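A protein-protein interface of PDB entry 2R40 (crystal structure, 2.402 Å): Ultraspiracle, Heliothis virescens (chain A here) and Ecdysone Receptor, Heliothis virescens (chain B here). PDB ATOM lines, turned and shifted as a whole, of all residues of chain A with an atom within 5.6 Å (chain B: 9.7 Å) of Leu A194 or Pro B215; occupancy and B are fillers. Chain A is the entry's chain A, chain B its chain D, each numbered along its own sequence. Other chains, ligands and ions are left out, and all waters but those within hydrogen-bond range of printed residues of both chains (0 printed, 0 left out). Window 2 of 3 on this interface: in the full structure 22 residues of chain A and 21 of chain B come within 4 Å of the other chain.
NH2 of Arg B216 lies within salt-bridge range of OE1 of Glu A190, 2.8 Å away. The side-chain carboxylate (OE2) of Glu A190 is in salt-bridge range of the side-chain amino group (NZ) of Lys B223.
The side-chain carboxylate (OD2) of Asp A197 is in salt-bridge range of the guanidinium group (NH2) of Arg A201, at 2.6 Å.
Val B219 touches Glu A190 (CG1 to CG, 3.6 Å). Phe A193 touches Gly B222. Lys B223 touches Phe A193. Pro B215 touches Leu A194 (O to CD1, 3.3 Å). CG2 of Val B219 touches CD2 of Leu A194, 3.7 Å away. Asp A197 touches Ala B218.
Arg A189 touches none of the printed residues of chain B. Leu A194 touches just these residues of chain B: Pro B215 and Val B219. Cys A195 touches none of the printed residues of chain B. Leu A196 touches none of the printed residues of chain B. Pro B215 touches just one residue of chain A: Leu A194. Of the printed residues of chain A, Arg B216 touches Glu A190 (2.8 Å). Printed residues of chain A within 4 Å of Val B219: Glu A190 and Leu A194. The nearest residue of chain B that does not touch Leu A194 is Arg B216 (4.2 Å). The nearest printed residue of chain A that does not touch Gly B222 is Arg A189 (5.8 Å).
Hydrophobic or aromatic side chains of chain A within 4 Å of the printed part of chain B: Phe A193 and Leu A194. Of the 15 printed residues of chain B, 6 touch a printed residue of chain A. Along chain B the printed residues that touch a printed residue of chain A span positions 215 to 223. Among the printed residues, 8 pairs touch across the chains.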
ATOM      1  N   ARG A 189     -20.863  -0.911 -20.764  1.00  0.00           N
ATOM      2  CA  ARG A 189     -19.949  -2.008 -20.429  1.00  0.00           C
ATOM      3  C   ARG A 189     -20.667  -3.320 -20.058  1.00  0.00           C
ATOM      4  O   ARG A 189     -20.247  -4.404 -20.477  1.00  0.00           O
ATOM      5  CB  ARG A 189     -18.972  -1.597 -19.318  1.00  0.00           C
ATOM      6  CG  ARG A 189     -17.978  -2.698 -18.981  1.00  0.00           C
ATOM      7  CD  ARG A 189     -17.030  -2.317 -17.878  1.00  0.00           C
ATOM      8  NE  ARG A 189     -15.775  -1.807 -18.433  1.00  0.00           N
ATOM      9  CZ  ARG A 189     -14.577  -1.996 -17.889  1.00  0.00           C
ATOM     10  NH1 ARG A 189     -14.445  -2.704 -16.768  1.00  0.00           N
ATOM     11  NH2 ARG A 189     -13.511  -1.476 -18.470  1.00  0.00           N
ATOM     12  N   GLU A 190     -21.728  -3.217 -19.261  1.00  0.00           N
ATOM     13  CA  GLU A 190     -22.555  -4.377 -18.898  1.00  0.00           C
ATOM     14  C   GLU A 190     -23.158  -5.050 -20.141  1.00  0.00           C
ATOM     15  O   GLU A 190     -23.208  -6.277 -20.231  1.00  0.00           O
ATOM     16  CB  GLU A 190     -23.642  -3.982 -17.880  1.00  0.00           C
ATOM     17  CG  GLU A 190     -23.055  -3.390 -16.574  1.00  0.00           C
ATOM     18  CD  GLU A 190     -24.109  -3.001 -15.535  1.00  0.00           C
ATOM     19  OE1 GLU A 190     -25.285  -3.402 -15.667  1.00  0.00           O
ATOM     20  OE2 GLU A 190     -23.751  -2.285 -14.571  1.00  0.00           O
ATOM     21  N   LYS A 191     -23.576  -4.234 -21.105  1.00  0.00           N
ATOM     22  CA  LYS A 191     -24.016  -4.714 -22.411  1.00  0.00           C
ATOM     23  C   LYS A 191     -22.939  -5.562 -23.090  1.00  0.00           C
ATOM     24  O   LYS A 191     -23.243  -6.599 -23.687  1.00  0.00           O
ATOM     25  CB  LYS A 191     -24.373  -3.526 -23.307  1.00  0.00           C
ATOM     26  CG  LYS A 191     -24.876  -3.898 -24.684  1.00  0.00           C
ATOM     27  CD  LYS A 191     -26.367  -4.195 -24.660  1.00  0.00           C
ATOM     28  CE  LYS A 191     -26.902  -4.503 -26.049  1.00  0.00           C
ATOM     29  NZ  LYS A 191     -26.589  -5.892 -26.486  1.00  0.00           N
ATOM     30  N   MET A 192     -21.689  -5.109 -22.990  1.00  0.00           N
ATOM     31  CA  MET A 192     -20.544  -5.805 -23.580  1.00  0.00           C
ATOM     32  C   MET A 192     -20.216  -7.123 -22.880  1.00  0.00           C
ATOM     33  O   MET A 192     -19.806  -8.069 -23.531  1.00  0.00           O
ATOM     34  CB  MET A 192     -19.292  -4.908 -23.622  1.00  0.00           C
ATOM     35  CG  MET A 192     -19.253  -3.861 -24.734  1.00  0.00           C
ATOM     36  SD  MET A 192     -19.795  -4.405 -26.371  1.00  0.00           S
ATOM     37  CE  MET A 192     -18.867  -5.931 -26.601  1.00  0.00           C
ATOM     38  N   PHE A 193     -20.379  -7.183 -21.561  1.00  0.00           N
ATOM     39  CA  PHE A 193     -20.211  -8.451 -20.831  1.00  0.00           C
ATOM     40  C   PHE A 193     -21.198  -9.512 -21.310  1.00  0.00           C
ATOM     41  O   PHE A 193     -20.832 -10.677 -21.468  1.00  0.00           O
ATOM     42  CB  PHE A 193     -20.369  -8.268 -19.311  1.00  0.00           C
ATOM     43  CG  PHE A 193     -19.237  -7.529 -18.662  1.00  0.00           C
ATOM     44  CD1 PHE A 193     -17.904  -7.835 -18.972  1.00  0.00           C
ATOM     45  CD2 PHE A 193     -19.491  -6.542 -17.712  1.00  0.00           C
ATOM     46  CE1 PHE A 193     -16.844  -7.149 -18.355  1.00  0.00           C
ATOM     47  CE2 PHE A 193     -18.435  -5.849 -17.096  1.00  0.00           C
ATOM     48  CZ  PHE A 193     -17.117  -6.157 -17.425  1.00  0.00           C
ATOM     49  N   LEU A 194     -22.443  -9.081 -21.533  1.00  0.00           N
ATOM     50  CA  LEU A 194     -23.521  -9.932 -22.026  1.00  0.00           C
ATOM     51  C   LEU A 194     -23.194 -10.457 -23.418  1.00  0.00           C
ATOM     52  O   LEU A 194     -23.216 -11.661 -23.647  1.00  0.00           O
ATOM     53  CB  LEU A 194     -24.861  -9.170 -22.053  1.00  0.00           C
ATOM     54  CG  LEU A 194     -25.992  -9.282 -21.009  1.00  0.00           C
ATOM     55  CD1 LEU A 194     -25.880 -10.502 -20.079  1.00  0.00           C
ATOM     56  CD2 LEU A 194     -26.190  -8.000 -20.199  1.00  0.00           C
ATOM     57  N   CYS A 195     -22.891  -9.541 -24.339  1.00  0.00           N
ATOM     58  CA  CYS A 195     -22.417  -9.880 -25.686  1.00  0.00           C
ATOM     59  C   CYS A 195     -21.258 -10.878 -25.690  1.00  0.00           C
ATOM     60  O   CYS A 195     -21.301 -11.885 -26.407  1.00  0.00           O
ATOM     61  CB  CYS A 195     -21.995  -8.617 -26.440  1.00  0.00           C
ATOM     62  SG  CYS A 195     -23.392  -7.595 -26.937  1.00  0.00           S
ATOM     63  N   LEU A 196     -20.233 -10.598 -24.892  1.00  0.00           N
ATOM     64  CA  LEU A 196     -19.056 -11.454 -24.834  1.00  0.00           C
ATOM     65  C   LEU A 196     -19.375 -12.854 -24.298  1.00  0.00           C
ATOM     66  O   LEU A 196     -18.924 -13.849 -24.869  1.00  0.00           O
ATOM     67  CB  LEU A 196     -17.930 -10.797 -24.023  1.00  0.00           C
ATOM     68  CG  LEU A 196     -16.598 -11.557 -23.977  1.00  0.00           C
ATOM     69  CD1 LEU A 196     -16.055 -11.824 -25.384  1.00  0.00           C
ATOM     70  CD2 LEU A 196     -15.567 -10.819 -23.137  1.00  0.00           C
ATOM     71  N   ASP A 197     -20.145 -12.915 -23.214  1.00  0.00           N
ATOM     72  CA  ASP A 197     -20.539 -14.182 -22.591  1.00  0.00           C
ATOM     73  C   ASP A 197     -21.425 -15.025 -23.527  1.00  0.00           C
ATOM     74  O   ASP A 197     -21.191 -16.226 -23.685  1.00  0.00           O
ATOM     75  CB  ASP A 197     -21.256 -13.912 -21.263  1.00  0.00           C
ATOM     76  CG  ASP A 197     -21.682 -15.178 -20.552  1.00  0.00           C
ATOM     77  OD1 ASP A 197     -20.888 -15.741 -19.768  1.00  0.00           O
ATOM     78  OD2 ASP A 197     -22.843 -15.591 -20.750  1.00  0.00           O
ATOM     79  N   GLU A 198     -22.429 -14.386 -24.137  1.00  0.00           N
ATOM     80  CA  GLU A 198     -23.285 -15.018 -25.143  1.00  0.00           C
ATOM     81  C   GLU A 198     -22.446 -15.675 -26.241  1.00  0.00           C
ATOM     82  O   GLU A 198     -22.615 -16.867 -26.527  1.00  0.00           O
ATOM     83  CB  GLU A 198     -24.266 -14.000 -25.749  1.00  0.00           C
ATOM     84  CG  GLU A 198     -25.277 -14.614 -26.717  1.00  0.00           C
ATOM     85  CD  GLU A 198     -26.201 -13.589 -27.375  1.00  0.00           C
ATOM     86  OE1 GLU A 198     -25.697 -12.693 -28.088  1.00  0.00           O
ATOM     87  OE2 GLU A 198     -27.438 -13.696 -27.194  1.00  0.00           O
ATOM     88  N   TYR A 199     -21.543 -14.893 -26.831  1.00  0.00           N
ATOM     89  CA  TYR A 199     -20.642 -15.356 -27.888  1.00  0.00           C
ATOM     90  C   TYR A 199     -19.780 -16.556 -27.478  1.00  0.00           C
ATOM     91  O   TYR A 199     -19.621 -17.498 -28.255  1.00  0.00           O
ATOM     92  CB  TYR A 199     -19.745 -14.204 -28.370  1.00  0.00           C
ATOM     93  CG  TYR A 199     -18.905 -14.567 -29.568  1.00  0.00           C
ATOM     94  CD1 TYR A 199     -19.408 -14.427 -30.859  1.00  0.00           C
ATOM     95  CD2 TYR A 199     -17.621 -15.079 -29.414  1.00  0.00           C
ATOM     96  CE1 TYR A 199     -18.656 -14.784 -31.966  1.00  0.00           C
ATOM     97  CE2 TYR A 199     -16.857 -15.434 -30.510  1.00  0.00           C
ATOM     98  CZ  TYR A 199     -17.380 -15.289 -31.788  1.00  0.00           C
ATOM     99  OH  TYR A 199     -16.621 -15.634 -32.890  1.00  0.00           O
ATOM    100  N   ARG A 201     -20.315 -18.846 -25.103  1.00  0.00           N
ATOM    101  CA  ARG A 201     -21.141 -20.038 -24.887  1.00  0.00           C
ATOM    102  C   ARG A 201     -21.620 -20.668 -26.192  1.00  0.00           C
ATOM    103  O   ARG A 201     -22.185 -21.763 -26.190  1.00  0.00           O
ATOM    104  CB  ARG A 201     -22.352 -19.707 -24.008  1.00  0.00           C
ATOM    105  CG  ARG A 201     -22.079 -19.783 -22.514  1.00  0.00           C
ATOM    106  CD  ARG A 201     -23.375 -19.736 -21.711  1.00  0.00           C
ATOM    107  NE  ARG A 201     -23.856 -18.367 -21.549  1.00  0.00           N
ATOM    108  CZ  ARG A 201     -24.832 -17.992 -20.726  1.00  0.00           C
ATOM    109  NH1 ARG A 201     -25.473 -18.877 -19.958  1.00  0.00           N
ATOM    110  NH2 ARG A 201     -25.173 -16.713 -20.672  1.00  0.00           N
ATOM    111  N   ILE B 207     -21.747 -17.689  -8.247  1.00  0.00           N
ATOM    112  CA  ILE B 207     -22.589 -16.575  -8.706  1.00  0.00           C
ATOM    113  C   ILE B 207     -23.872 -17.087  -9.358  1.00  0.00           C
ATOM    114  O   ILE B 207     -24.958 -16.578  -9.066  1.00  0.00           O
ATOM    115  CB  ILE B 207     -21.832 -15.601  -9.653  1.00  0.00           C
ATOM    116  CG1 ILE B 207     -20.747 -14.841  -8.879  1.00  0.00           C
ATOM    117  CG2 ILE B 207     -22.818 -14.625 -10.324  1.00  0.00           C
ATOM    118  CD1 ILE B 207     -19.735 -14.112  -9.758  1.00  0.00           C
ATOM    119  N   LEU B 208     -23.743 -18.103 -10.214  1.00  0.00           N
ATOM    120  CA  LEU B 208     -24.903 -18.779 -10.831  1.00  0.00           C
ATOM    121  C   LEU B 208     -25.902 -19.294  -9.801  1.00  0.00           C
ATOM    122  O   LEU B 208     -27.124 -19.215 -10.011  1.00  0.00           O
ATOM    123  CB  LEU B 208     -24.456 -19.921 -11.754  1.00  0.00           C
ATOM    124  CG  LEU B 208     -23.729 -19.503 -13.043  1.00  0.00           C
ATOM    125  CD1 LEU B 208     -22.886 -20.647 -13.596  1.00  0.00           C
ATOM    126  CD2 LEU B 208     -24.714 -18.996 -14.102  1.00  0.00           C
ATOM    127  N   ASN B 211     -28.082 -16.344  -8.171  1.00  0.00           N
ATOM    128  CA  ASN B 211     -28.990 -15.585  -9.042  1.00  0.00           C
ATOM    129  C   ASN B 211     -29.824 -16.455  -9.981  1.00  0.00           C
ATOM    130  O   ASN B 211     -30.366 -15.956 -10.973  1.00  0.00           O
ATOM    131  CB  ASN B 211     -28.208 -14.562  -9.874  1.00  0.00           C
ATOM    132  CG  ASN B 211     -27.272 -13.716  -9.036  1.00  0.00           C
ATOM    133  OD1 ASN B 211     -27.665 -12.682  -8.495  1.00  0.00           O
ATOM    134  ND2 ASN B 211     -26.025 -14.147  -8.932  1.00  0.00           N
ATOM    135  N   SER B 212     -29.915 -17.752  -9.662  1.00  0.00           N
ATOM    136  CA  SER B 212     -30.686 -18.743 -10.424  1.00  0.00           C
ATOM    137  C   SER B 212     -30.321 -18.811 -11.916  1.00  0.00           C
ATOM    138  O   SER B 212     -31.185 -19.075 -12.770  1.00  0.00           O
ATOM    139  CB  SER B 212     -32.191 -18.526 -10.228  1.00  0.00           C
ATOM    140  OG  SER B 212     -32.481 -18.378  -8.834  1.00  0.00           O
ATOM    141  N   ALA B 213     -29.040 -18.573 -12.206  1.00  0.00           N
ATOM    142  CA  ALA B 213     -28.465 -18.699 -13.554  1.00  0.00           C
ATOM    143  C   ALA B 213     -29.101 -17.805 -14.631  1.00  0.00           C
ATOM    144  O   ALA B 213     -29.308 -18.244 -15.773  1.00  0.00           O
ATOM    145  CB  ALA B 213     -28.458 -20.181 -14.003  1.00  0.00           C
ATOM    146  N   SER B 214     -29.426 -16.562 -14.268  1.00  0.00           N
ATOM    147  CA  SER B 214     -29.919 -15.578 -15.245  1.00  0.00           C
ATOM    148  C   SER B 214     -28.727 -14.939 -15.998  1.00  0.00           C
ATOM    149  O   SER B 214     -27.581 -15.053 -15.545  1.00  0.00           O
ATOM    150  CB  SER B 214     -30.762 -14.502 -14.553  1.00  0.00           C
ATOM    151  OG  SER B 214     -29.984 -13.764 -13.617  1.00  0.00           O
ATOM    152  N   PRO B 215     -28.992 -14.289 -17.157  1.00  0.00           N
ATOM    153  CA  PRO B 215     -27.968 -13.613 -17.962  1.00  0.00           C
ATOM    154  C   PRO B 215     -27.060 -12.656 -17.187  1.00  0.00           C
ATOM    155  O   PRO B 215     -25.874 -12.551 -17.515  1.00  0.00           O
ATOM    156  CB  PRO B 215     -28.799 -12.829 -18.984  1.00  0.00           C
ATOM    157  CG  PRO B 215     -29.993 -13.654 -19.171  1.00  0.00           C
ATOM    158  CD  PRO B 215     -30.319 -14.195 -17.799  1.00  0.00           C
ATOM    159  N   ARG B 216     -27.602 -11.981 -16.170  1.00  0.00           N
ATOM    160  CA  ARG B 216     -26.842 -10.970 -15.408  1.00  0.00           C
ATOM    161  C   ARG B 216     -25.710 -11.531 -14.535  1.00  0.00           C
ATOM    162  O   ARG B 216     -24.890 -10.769 -14.019  1.00  0.00           O
ATOM    163  CB  ARG B 216     -27.781 -10.056 -14.601  1.00  0.00           C
ATOM    164  CG  ARG B 216     -28.698  -9.158 -15.472  1.00  0.00           C
ATOM    165  CD  ARG B 216     -27.894  -8.184 -16.370  1.00  0.00           C
ATOM    166  NE  ARG B 216     -27.820  -6.803 -15.869  1.00  0.00           N
ATOM    167  CZ  ARG B 216     -27.113  -6.391 -14.815  1.00  0.00           C
ATOM    168  NH1 ARG B 216     -26.402  -7.244 -14.087  1.00  0.00           N
ATOM    169  NH2 ARG B 216     -27.131  -5.107 -14.473  1.00  0.00           N
ATOM    170  N   CYS B 217     -25.655 -12.855 -14.395  1.00  0.00           N
ATOM    171  CA  CYS B 217     -24.519 -13.538 -13.766  1.00  0.00           C
ATOM    172  C   CYS B 217     -23.178 -13.225 -14.456  1.00  0.00           C
ATOM    173  O   CYS B 217     -22.145 -13.153 -13.797  1.00  0.00           O
ATOM    174  CB  CYS B 217     -24.746 -15.052 -13.733  1.00  0.00           C
ATOM    175  SG  CYS B 217     -25.865 -15.597 -12.433  1.00  0.00           S
ATOM    176  N   ALA B 218     -23.209 -13.033 -15.772  1.00  0.00           N
ATOM    177  CA  ALA B 218     -22.029 -12.638 -16.541  1.00  0.00           C
ATOM    178  C   ALA B 218     -21.596 -11.201 -16.233  1.00  0.00           C
ATOM    179  O   ALA B 218     -20.403 -10.894 -16.244  1.00  0.00           O
ATOM    180  CB  ALA B 218     -22.286 -12.804 -18.031  1.00  0.00           C
ATOM    181  N   VAL B 219     -22.571 -10.330 -15.965  1.00  0.00           N
ATOM    182  CA  VAL B 219     -22.294  -8.924 -15.633  1.00  0.00           C
ATOM    183  C   VAL B 219     -21.645  -8.819 -14.251  1.00  0.00           C
ATOM    184  O   VAL B 219     -20.616  -8.154 -14.080  1.00  0.00           O
ATOM    185  CB  VAL B 219     -23.568  -8.055 -15.732  1.00  0.00           C
ATOM    186  CG1 VAL B 219     -23.327  -6.665 -15.190  1.00  0.00           C
ATOM    187  CG2 VAL B 219     -24.020  -7.972 -17.159  1.00  0.00           C
ATOM    188  N   ILE B 220     -22.231  -9.515 -13.282  1.00  0.00           N
ATOM    189  CA  ILE B 220     -21.692  -9.578 -11.921  1.00  0.00           C
ATOM    190  C   ILE B 220     -20.291 -10.186 -11.930  1.00  0.00           C
ATOM    191  O   ILE B 220     -19.399  -9.691 -11.260  1.00  0.00           O
ATOM    192  CB  ILE B 220     -22.653 -10.369 -10.977  1.00  0.00           C
ATOM    193  CG1 ILE B 220     -24.041  -9.712 -10.963  1.00  0.00           C
ATOM    194  CG2 ILE B 220     -22.089 -10.477  -9.567  1.00  0.00           C
ATOM    195  CD1 ILE B 220     -25.187 -10.618 -10.491  1.00  0.00           C
ATOM    196  N   PHE B 221     -20.101 -11.249 -12.707  1.00  0.00           N
ATOM    197  CA  PHE B 221     -18.812 -11.948 -12.800  1.00  0.00           C
ATOM    198  C   PHE B 221     -17.762 -11.071 -13.515  1.00  0.00           C
ATOM    199  O   PHE B 221     -16.611 -10.974 -13.075  1.00  0.00           O
ATOM    200  CB  PHE B 221     -19.042 -13.304 -13.497  1.00  0.00           C
ATOM    201  CG  PHE B 221     -17.844 -14.226 -13.510  1.00  0.00           C
ATOM    202  CD1 PHE B 221     -16.975 -14.300 -12.427  1.00  0.00           C
ATOM    203  CD2 PHE B 221     -17.624 -15.064 -14.608  1.00  0.00           C
ATOM    204  CE1 PHE B 221     -15.881 -15.162 -12.438  1.00  0.00           C
ATOM    205  CE2 PHE B 221     -16.539 -15.928 -14.631  1.00  0.00           C
ATOM    206  CZ  PHE B 221     -15.656 -15.974 -13.534  1.00  0.00           C
ATOM    207  N   GLY B 222     -18.180 -10.409 -14.593  1.00  0.00           N
ATOM    208  CA  GLY B 222     -17.346  -9.441 -15.316  1.00  0.00           C
ATOM    209  C   GLY B 222     -16.891  -8.235 -14.498  1.00  0.00           C
ATOM    210  O   GLY B 222     -15.723  -7.861 -14.562  1.00  0.00           O
ATOM    211  N   LYS B 223     -17.811  -7.622 -13.741  1.00  0.00           N
ATOM    212  CA  LYS B 223     -17.483  -6.488 -12.837  1.00  0.00           C
ATOM    213  C   LYS B 223     -16.460  -6.880 -11.790  1.00  0.00           C
ATOM    214  O   LYS B 223     -15.504  -6.128 -11.535  1.00  0.00           O
ATOM    215  CB  LYS B 223     -18.729  -5.912 -12.152  1.00  0.00           C
ATOM    216  CG  LYS B 223     -19.479  -4.890 -12.993  1.00  0.00           C
ATOM    217  CD  LYS B 223     -20.987  -4.826 -12.674  1.00  0.00           C
ATOM    218  CE  LYS B 223     -21.329  -3.766 -11.605  1.00  0.00           C
ATOM    219  NZ  LYS B 223     -22.825  -3.676 -11.289  1.00  0.00           N
